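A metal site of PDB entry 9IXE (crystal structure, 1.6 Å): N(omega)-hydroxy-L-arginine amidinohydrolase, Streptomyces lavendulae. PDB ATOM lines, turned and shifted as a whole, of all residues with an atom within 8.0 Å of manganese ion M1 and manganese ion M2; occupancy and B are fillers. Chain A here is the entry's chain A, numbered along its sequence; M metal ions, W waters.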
ATOM      1  N   MET A  18       3.419 -18.186  17.646  1.00  0.00           N
ATOM      2  CA  MET A  18       3.505 -18.553  19.052  1.00  0.00           C
ATOM      3  C   MET A  18       2.334 -19.401  19.524  1.00  0.00           C
ATOM      4  O   MET A  18       2.504 -20.247  20.402  1.00  0.00           O
ATOM      5  CB  MET A  18       3.680 -17.298  19.914  1.00  0.00           C
ATOM      6  CG  MET A  18       5.112 -16.717  19.836  1.00  0.00           C
ATOM      7  SD  MET A  18       5.354 -15.329  20.957  1.00  0.00           S
ATOM      8  CE  MET A  18       6.994 -14.777  20.468  1.00  0.00           C
ATOM      9  N   THR A  85       1.854 -16.587  24.715  1.00  0.00           N
ATOM     10  CA  THR A  85       2.599 -15.379  25.062  1.00  0.00           C
ATOM     11  C   THR A  85       2.766 -15.261  26.570  1.00  0.00           C
ATOM     12  O   THR A  85       2.022 -15.866  27.350  1.00  0.00           O
ATOM     13  CB  THR A  85       1.906 -14.107  24.550  1.00  0.00           C
ATOM     14  OG1 THR A  85       0.627 -13.987  25.201  1.00  0.00           O
ATOM     15  CG2 THR A  85       1.743 -14.141  23.032  1.00  0.00           C
ATOM     16  N   CYS A  86       3.756 -14.452  26.965  1.00  0.00           N
ATOM     17  CA  CYS A  86       3.937 -14.103  28.377  1.00  0.00           C
ATOM     18  C   CYS A  86       2.690 -13.459  28.954  1.00  0.00           C
ATOM     19  O   CYS A  86       2.404 -13.626  30.142  1.00  0.00           O
ATOM     20  CB  CYS A  86       5.124 -13.164  28.569  1.00  0.00           C
ATOM     21  SG  CYS A  86       6.686 -14.075  28.519  1.00  0.00           S
ATOM     22  N   SER A  87       1.932 -12.718  28.138  1.00  0.00           N
ATOM     23  CA  SER A  87       0.751 -12.022  28.641  1.00  0.00           C
ATOM     24  C   SER A  87      -0.323 -12.929  29.198  1.00  0.00           C
ATOM     25  O   SER A  87      -1.140 -12.458  30.005  1.00  0.00           O
ATOM     26  CB  SER A  87       0.145 -11.097  27.580  1.00  0.00           C
ATOM     27  OG  SER A  87       1.102 -10.173  27.117  1.00  0.00           O
ATOM     28  N   TYR A 107      11.021 -15.381  37.003  1.00  0.00           N
ATOM     29  CA  TYR A 107      10.520 -14.892  35.728  1.00  0.00           C
ATOM     30  C   TYR A 107      11.718 -14.905  34.790  1.00  0.00           C
ATOM     31  O   TYR A 107      12.565 -13.997  34.820  1.00  0.00           O
ATOM     32  CB  TYR A 107       9.901 -13.504  35.874  1.00  0.00           C
ATOM     33  CG  TYR A 107       8.996 -13.086  34.731  1.00  0.00           C
ATOM     34  CD1 TYR A 107       9.535 -12.558  33.566  1.00  0.00           C
ATOM     35  CD2 TYR A 107       7.613 -13.204  34.831  1.00  0.00           C
ATOM     36  CE1 TYR A 107       8.712 -12.157  32.497  1.00  0.00           C
ATOM     37  CE2 TYR A 107       6.778 -12.791  33.796  1.00  0.00           C
ATOM     38  CZ  TYR A 107       7.337 -12.272  32.626  1.00  0.00           C
ATOM     39  OH  TYR A 107       6.500 -11.872  31.609  1.00  0.00           O
ATOM     40  N   ILE A 108      11.829 -15.953  33.992  1.00  0.00           N
ATOM     41  CA  ILE A 108      13.037 -16.238  33.231  1.00  0.00           C
ATOM     42  C   ILE A 108      12.800 -15.700  31.817  1.00  0.00           C
ATOM     43  O   ILE A 108      11.968 -16.223  31.079  1.00  0.00           O
ATOM     44  CB  ILE A 108      13.372 -17.729  33.242  1.00  0.00           C
ATOM     45  CG1 ILE A 108      13.376 -18.259  34.683  1.00  0.00           C
ATOM     46  CG2 ILE A 108      14.679 -17.989  32.498  1.00  0.00           C
ATOM     47  CD1 ILE A 108      13.754 -19.720  34.790  1.00  0.00           C
ATOM     48  N   ASP A 109      13.559 -14.680  31.420  1.00  0.00           N
ATOM     49  CA  ASP A 109      13.167 -13.885  30.251  1.00  0.00           C
ATOM     50  C   ASP A 109      14.360 -13.030  29.849  1.00  0.00           C
ATOM     51  O   ASP A 109      15.064 -12.514  30.725  1.00  0.00           O
ATOM     52  CB  ASP A 109      11.945 -13.010  30.622  1.00  0.00           C
ATOM     53  CG  ASP A 109      11.173 -12.470  29.421  1.00  0.00           C
ATOM     54  OD1 ASP A 109      11.783 -11.974  28.442  1.00  0.00           O
ATOM     55  OD2 ASP A 109       9.911 -12.499  29.486  1.00  0.00           O
ATOM     56  N   GLY A 110      14.603 -12.895  28.548  1.00  0.00           N
ATOM     57  CA  GLY A 110      15.621 -11.947  28.136  1.00  0.00           C
ATOM     58  C   GLY A 110      15.247 -10.500  28.403  1.00  0.00           C
ATOM     59  O   GLY A 110      16.130  -9.632  28.404  1.00  0.00           O
ATOM     60  N   HIS A 111      13.956 -10.245  28.624  1.00  0.00           N
ATOM     61  CA  HIS A 111      13.395  -8.943  28.909  1.00  0.00           C
ATOM     62  C   HIS A 111      12.986  -8.837  30.369  1.00  0.00           C
ATOM     63  O   HIS A 111      12.827  -9.844  31.072  1.00  0.00           O
ATOM     64  CB  HIS A 111      12.166  -8.684  28.039  1.00  0.00           C
ATOM     65  CG  HIS A 111      12.447  -8.741  26.575  1.00  0.00           C
ATOM     66  ND1 HIS A 111      12.321  -9.897  25.843  1.00  0.00           N
ATOM     67  CD2 HIS A 111      12.854  -7.779  25.710  1.00  0.00           C
ATOM     68  CE1 HIS A 111      12.650  -9.648  24.577  1.00  0.00           C
ATOM     69  NE2 HIS A 111      12.947  -8.371  24.468  1.00  0.00           N
ATOM     70  N   GLY A 112      12.712  -7.604  30.792  1.00  0.00           N
ATOM     71  CA  GLY A 112      12.162  -7.371  32.123  1.00  0.00           C
ATOM     72  C   GLY A 112      10.645  -7.492  32.203  1.00  0.00           C
ATOM     73  O   GLY A 112      10.103  -7.773  33.281  1.00  0.00           O
ATOM     74  N   ASP A 113       9.963  -7.262  31.071  1.00  0.00           N
ATOM     75  CA  ASP A 113       8.496  -7.274  31.005  1.00  0.00           C
ATOM     76  C   ASP A 113       7.902  -6.454  32.155  1.00  0.00           C
ATOM     77  O   ASP A 113       6.900  -6.830  32.773  1.00  0.00           O
ATOM     78  CB  ASP A 113       7.935  -8.708  30.998  1.00  0.00           C
ATOM     79  CG  ASP A 113       8.243  -9.459  29.711  1.00  0.00           C
ATOM     80  OD1 ASP A 113       8.946  -8.904  28.843  1.00  0.00           O
ATOM     81  OD2 ASP A 113       7.776 -10.606  29.573  1.00  0.00           O
ATOM     82  N   TYR A 124       3.145  -2.657  23.755  1.00  0.00           N
ATOM     83  CA  TYR A 124       2.963  -4.106  23.724  1.00  0.00           C
ATOM     84  C   TYR A 124       2.648  -4.669  25.109  1.00  0.00           C
ATOM     85  O   TYR A 124       3.425  -4.475  26.065  1.00  0.00           O
ATOM     86  CB  TYR A 124       4.206  -4.771  23.143  1.00  0.00           C
ATOM     87  CG  TYR A 124       4.099  -6.280  22.999  1.00  0.00           C
ATOM     88  CD1 TYR A 124       2.928  -6.880  22.546  1.00  0.00           C
ATOM     89  CD2 TYR A 124       5.180  -7.082  23.314  1.00  0.00           C
ATOM     90  CE1 TYR A 124       2.839  -8.268  22.405  1.00  0.00           C
ATOM     91  CE2 TYR A 124       5.090  -8.467  23.190  1.00  0.00           C
ATOM     92  CZ  TYR A 124       3.924  -9.046  22.741  1.00  0.00           C
ATOM     93  OH  TYR A 124       3.840 -10.410  22.621  1.00  0.00           O
ATOM     94  N   LEU A 125       1.521  -5.379  25.199  1.00  0.00           N
ATOM     95  CA  LEU A 125       1.090  -5.971  26.468  1.00  0.00           C
ATOM     96  C   LEU A 125       2.136  -6.920  27.031  1.00  0.00           C
ATOM     97  O   LEU A 125       2.306  -6.999  28.255  1.00  0.00           O
ATOM     98  CB  LEU A 125      -0.243  -6.704  26.270  1.00  0.00           C
ATOM     99  CG  LEU A 125      -0.934  -7.273  27.506  1.00  0.00           C
ATOM    100  CD1 LEU A 125      -1.305  -6.156  28.481  1.00  0.00           C
ATOM    101  CD2 LEU A 125      -2.162  -8.097  27.119  1.00  0.00           C
ATOM    102  N   GLY A 126       2.815  -7.655  26.159  1.00  0.00           N
ATOM    103  CA  GLY A 126       3.807  -8.613  26.624  1.00  0.00           C
ATOM    104  C   GLY A 126       4.959  -7.971  27.368  1.00  0.00           C
ATOM    105  O   GLY A 126       5.597  -8.618  28.205  1.00  0.00           O
ATOM    106  N   GLY A 127       5.259  -6.715  27.087  1.00  0.00           N
ATOM    107  CA  GLY A 127       6.277  -6.041  27.859  1.00  0.00           C
ATOM    108  C   GLY A 127       5.796  -5.463  29.174  1.00  0.00           C
ATOM    109  O   GLY A 127       6.547  -4.727  29.822  1.00  0.00           O
ATOM    110  N   MET A 128       4.562  -5.789  29.577  1.00  0.00           N
ATOM    111  CA  MET A 128       3.932  -5.192  30.752  1.00  0.00           C
ATOM    112  C   MET A 128       3.439  -6.257  31.726  1.00  0.00           C
ATOM    113  O   MET A 128       2.665  -5.940  32.646  1.00  0.00           O
ATOM    114  CB  MET A 128       2.773  -4.259  30.367  1.00  0.00           C
ATOM    115  CG  MET A 128       3.137  -3.243  29.279  1.00  0.00           C
ATOM    116  SD  MET A 128       1.690  -2.510  28.405  1.00  0.00           S
ATOM    117  CE  MET A 128       0.902  -1.670  29.751  1.00  0.00           C
ATOM    118  N   VAL A 129       3.901  -7.496  31.571  1.00  0.00           N
ATOM    119  CA  VAL A 129       3.307  -8.631  32.277  1.00  0.00           C
ATOM    120  C   VAL A 129       3.702  -8.635  33.754  1.00  0.00           C
ATOM    121  O   VAL A 129       2.850  -8.789  34.628  1.00  0.00           O
ATOM    122  CB  VAL A 129       3.720  -9.950  31.607  1.00  0.00           C
ATOM    123  CG1 VAL A 129       3.218 -11.149  32.411  1.00  0.00           C
ATOM    124  CG2 VAL A 129       3.173 -10.005  30.169  1.00  0.00           C
ATOM    125  N   LEU A 130       4.997  -8.551  34.056  1.00  0.00           N
ATOM    126  CA  LEU A 130       5.417  -8.687  35.450  1.00  0.00           C
ATOM    127  C   LEU A 130       5.002  -7.479  36.267  1.00  0.00           C
ATOM    128  O   LEU A 130       4.592  -7.622  37.425  1.00  0.00           O
ATOM    129  CB  LEU A 130       6.932  -8.939  35.530  1.00  0.00           C
ATOM    130  CG  LEU A 130       7.541  -9.242  36.913  1.00  0.00           C
ATOM    131  CD1 LEU A 130       6.863 -10.431  37.613  1.00  0.00           C
ATOM    132  CD2 LEU A 130       9.043  -9.498  36.773  1.00  0.00           C
ATOM    133  N   LEU A 152      13.776 -11.688  38.253  1.00  0.00           N
ATOM    134  CA  LEU A 152      14.045 -11.784  36.817  1.00  0.00           C
ATOM    135  C   LEU A 152      15.336 -12.563  36.623  1.00  0.00           C
ATOM    136  O   LEU A 152      16.354 -12.242  37.245  1.00  0.00           O
ATOM    137  CB  LEU A 152      14.179 -10.394  36.203  1.00  0.00           C
ATOM    138  CG  LEU A 152      12.867  -9.668  35.937  1.00  0.00           C
ATOM    139  CD1 LEU A 152      13.120  -8.174  35.720  1.00  0.00           C
ATOM    140  CD2 LEU A 152      12.139 -10.297  34.754  1.00  0.00           C
ATOM    141  N   SER A 155      17.605 -11.781  32.296  1.00  0.00           N
ATOM    142  CA  SER A 155      17.309 -10.501  31.654  1.00  0.00           C
ATOM    143  C   SER A 155      18.584  -9.699  31.441  1.00  0.00           C
ATOM    144  O   SER A 155      19.501  -9.726  32.270  1.00  0.00           O
ATOM    145  CB  SER A 155      16.325  -9.714  32.530  1.00  0.00           C
ATOM    146  OG  SER A 155      15.223 -10.530  32.936  1.00  0.00           O
ATOM    147  N   HIS A 196       8.381 -19.227  35.408  1.00  0.00           N
ATOM    148  CA  HIS A 196       7.802 -18.694  34.172  1.00  0.00           C
ATOM    149  C   HIS A 196       8.955 -18.498  33.179  1.00  0.00           C
ATOM    150  O   HIS A 196       9.914 -17.804  33.493  1.00  0.00           O
ATOM    151  CB  HIS A 196       7.091 -17.362  34.462  1.00  0.00           C
ATOM    152  CG  HIS A 196       6.720 -16.582  33.237  1.00  0.00           C
ATOM    153  ND1 HIS A 196       5.405 -16.351  32.880  1.00  0.00           N
ATOM    154  CD2 HIS A 196       7.481 -15.974  32.301  1.00  0.00           C
ATOM    155  CE1 HIS A 196       5.379 -15.631  31.770  1.00  0.00           C
ATOM    156  NE2 HIS A 196       6.624 -15.404  31.385  1.00  0.00           N
ATOM    157  N   ILE A 197       8.853 -19.095  31.990  1.00  0.00           N
ATOM    158  CA  ILE A 197       9.931 -19.016  30.997  1.00  0.00           C
ATOM    159  C   ILE A 197       9.423 -18.424  29.692  1.00  0.00           C
ATOM    160  O   ILE A 197       8.449 -18.906  29.114  1.00  0.00           O
ATOM    161  CB  ILE A 197      10.545 -20.390  30.733  1.00  0.00           C
ATOM    162  CG1 ILE A 197      11.164 -20.906  32.008  1.00  0.00           C
ATOM    163  CG2 ILE A 197      11.625 -20.247  29.622  1.00  0.00           C
ATOM    164  CD1 ILE A 197      11.800 -22.267  31.866  1.00  0.00           C
ATOM    165  N   ASP A 198      10.148 -17.405  29.206  1.00  0.00           N
ATOM    166  CA  ASP A 198      10.053 -16.830  27.874  1.00  0.00           C
ATOM    167  C   ASP A 198      11.285 -17.300  27.129  1.00  0.00           C
ATOM    168  O   ASP A 198      12.416 -16.981  27.539  1.00  0.00           O
ATOM    169  CB  ASP A 198      10.006 -15.301  28.000  1.00  0.00           C
ATOM    170  CG  ASP A 198       9.968 -14.557  26.666  1.00  0.00           C
ATOM    171  OD1 ASP A 198      10.318 -15.113  25.607  1.00  0.00           O
ATOM    172  OD2 ASP A 198       9.568 -13.369  26.724  1.00  0.00           O
ATOM    173  N   TRP A 199      11.099 -18.066  26.046  1.00  0.00           N
ATOM    174  CA  TRP A 199      12.243 -18.684  25.399  1.00  0.00           C
ATOM    175  C   TRP A 199      13.221 -17.688  24.771  1.00  0.00           C
ATOM    176  O   TRP A 199      14.325 -18.098  24.423  1.00  0.00           O
ATOM    177  CB  TRP A 199      11.784 -19.691  24.332  1.00  0.00           C
ATOM    178  CG  TRP A 199      11.015 -20.850  24.943  1.00  0.00           C
ATOM    179  CD1 TRP A 199       9.723 -21.219  24.646  1.00  0.00           C
ATOM    180  CD2 TRP A 199      11.473 -21.768  25.942  1.00  0.00           C
ATOM    181  NE1 TRP A 199       9.359 -22.305  25.382  1.00  0.00           N
ATOM    182  CE2 TRP A 199      10.413 -22.660  26.207  1.00  0.00           C
ATOM    183  CE3 TRP A 199      12.675 -21.909  26.659  1.00  0.00           C
ATOM    184  CZ2 TRP A 199      10.511 -23.703  27.141  1.00  0.00           C
ATOM    185  CZ3 TRP A 199      12.773 -22.938  27.591  1.00  0.00           C
ATOM    186  CH2 TRP A 199      11.686 -23.810  27.830  1.00  0.00           C
ATOM    187  N   ASP A 200      12.868 -16.402  24.644  1.00  0.00           N
ATOM    188  CA  ASP A 200      13.872 -15.480  24.125  1.00  0.00           C
ATOM    189  C   ASP A 200      15.026 -15.244  25.115  1.00  0.00           C
ATOM    190  O   ASP A 200      15.973 -14.541  24.771  1.00  0.00           O
ATOM    191  CB  ASP A 200      13.237 -14.147  23.671  1.00  0.00           C
ATOM    192  CG  ASP A 200      12.581 -13.346  24.804  1.00  0.00           C
ATOM    193  OD1 ASP A 200      13.057 -13.406  25.957  1.00  0.00           O
ATOM    194  OD2 ASP A 200      11.615 -12.582  24.526  1.00  0.00           O
ATOM    195  N   VAL A 201      14.969 -15.842  26.313  1.00  0.00           N
ATOM    196  CA  VAL A 201      16.087 -15.791  27.231  1.00  0.00           C
ATOM    197  C   VAL A 201      17.274 -16.578  26.680  1.00  0.00           C
ATOM    198  O   VAL A 201      18.417 -16.345  27.089  1.00  0.00           O
ATOM    199  CB  VAL A 201      15.659 -16.319  28.620  1.00  0.00           C
ATOM    200  CG1 VAL A 201      15.490 -17.852  28.605  1.00  0.00           C
ATOM    201  CG2 VAL A 201      16.635 -15.885  29.705  1.00  0.00           C
ATOM    202  N   ALA A 240       6.468 -20.276  27.638  1.00  0.00           N
ATOM    203  CA  ALA A 240       5.876 -19.256  26.780  1.00  0.00           C
ATOM    204  C   ALA A 240       6.806 -18.838  25.644  1.00  0.00           C
ATOM    205  O   ALA A 240       8.040 -18.878  25.768  1.00  0.00           O
ATOM    206  CB  ALA A 240       5.496 -18.023  27.590  1.00  0.00           C
ATOM    207  N   GLU A 241       6.184 -18.475  24.521  1.00  0.00           N
ATOM    208  CA  GLU A 241       6.810 -17.706  23.439  1.00  0.00           C
ATOM    209  C   GLU A 241       7.806 -18.543  22.628  1.00  0.00           C
ATOM    210  O   GLU A 241       8.916 -18.095  22.307  1.00  0.00           O
ATOM    211  CB  GLU A 241       7.466 -16.421  23.984  1.00  0.00           C
ATOM    212  CG  GLU A 241       6.512 -15.598  24.880  1.00  0.00           C
ATOM    213  CD  GLU A 241       6.380 -14.126  24.487  1.00  0.00           C
ATOM    214  OE1 GLU A 241       7.185 -13.643  23.660  1.00  0.00           O
ATOM    215  OE2 GLU A 241       5.493 -13.470  25.079  1.00  0.00           O
HETATM  216 MN    MN M   1       8.308 -12.212  28.079  1.00  0.00          MN
HETATM  217 MN    MN M   2      11.253 -11.712  26.437  1.00  0.00          MN
HETATM  218  O   HOH W   1       6.893 -11.408  26.673  1.00  0.00           O
HETATM  219  O   HOH W   2       9.497 -10.462  26.802  1.00  0.00           O
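Manganese ion M2 is bound by OD1 of Asp 109 (2.1 Å), OD2 of Asp 200 (2.1 Å), water W2 (2.2 Å), ND1 of His 111 (2.2 Å), OD2 of Asp 198 (2.4 Å) and OD1 of Asp 200 (2.5 Å).
Water W1 bridges the side-chain carboxylate of Glu 241 (3.0 Å) and the backbone carbonyl oxygen of Gly 126 (3.4 Å).
The side-chain carboxylate of Asp 200 sits close to the backbone NH of Gly 110, at 3.1 Å. The backbone carbonyl oxygen (O) of Asp 113 lies within hydrogen-bond range of the backbone NH (N) of Leu 130 (2.9 Å). The side-chain hydroxyl of Tyr 107 sits close to the side-chain carboxylate of Asp 113. The backbone carbonyl oxygen (O) of Asp 109 lies within hydrogen-bond range of the side-chain hydroxyl (OG) of Ser 155. SG of Cys 86 sits close to OH of Tyr 107. The side-chain hydroxyl (OG) of Ser 155 lies within hydrogen-bond range of the backbone carbonyl oxygen (O) of His 111, 3.1 Å away. The backbone carbonyl oxygen of Asp 113 lies within hydrogen-bond range of the backbone NH of Val 129, at 3.3 Å. N of Asp 198 is in hydrogen-bond range of O of Ile 108 (2.9 Å).
Within 4 Å of manganese ion M2: Asp 109, His 111, Asp 198 and Asp 200.
Merely in contact with manganese ion M1: Tyr 107 (3.98 Å). Within 4 Å of manganese ion M1: Cys 86, Tyr 107, Asp 109, Asp 113 and Asp 198.
Water W1 is bound to manganese ion M1. OD2 of Asp 109 binds manganese ion M1. Manganese ion M1 is bound by the side-chain carboxylate (OD2) of Asp 198. The side-chain carboxylate (OD2) of Asp 113 binds manganese ion M1 (2.3 Å). Water W2 is bound to manganese ion M1 (2.5 Å). Manganese ion M1 is bound by the side-chain sulfur (SG) of Cys 86, 2.5 Å away.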
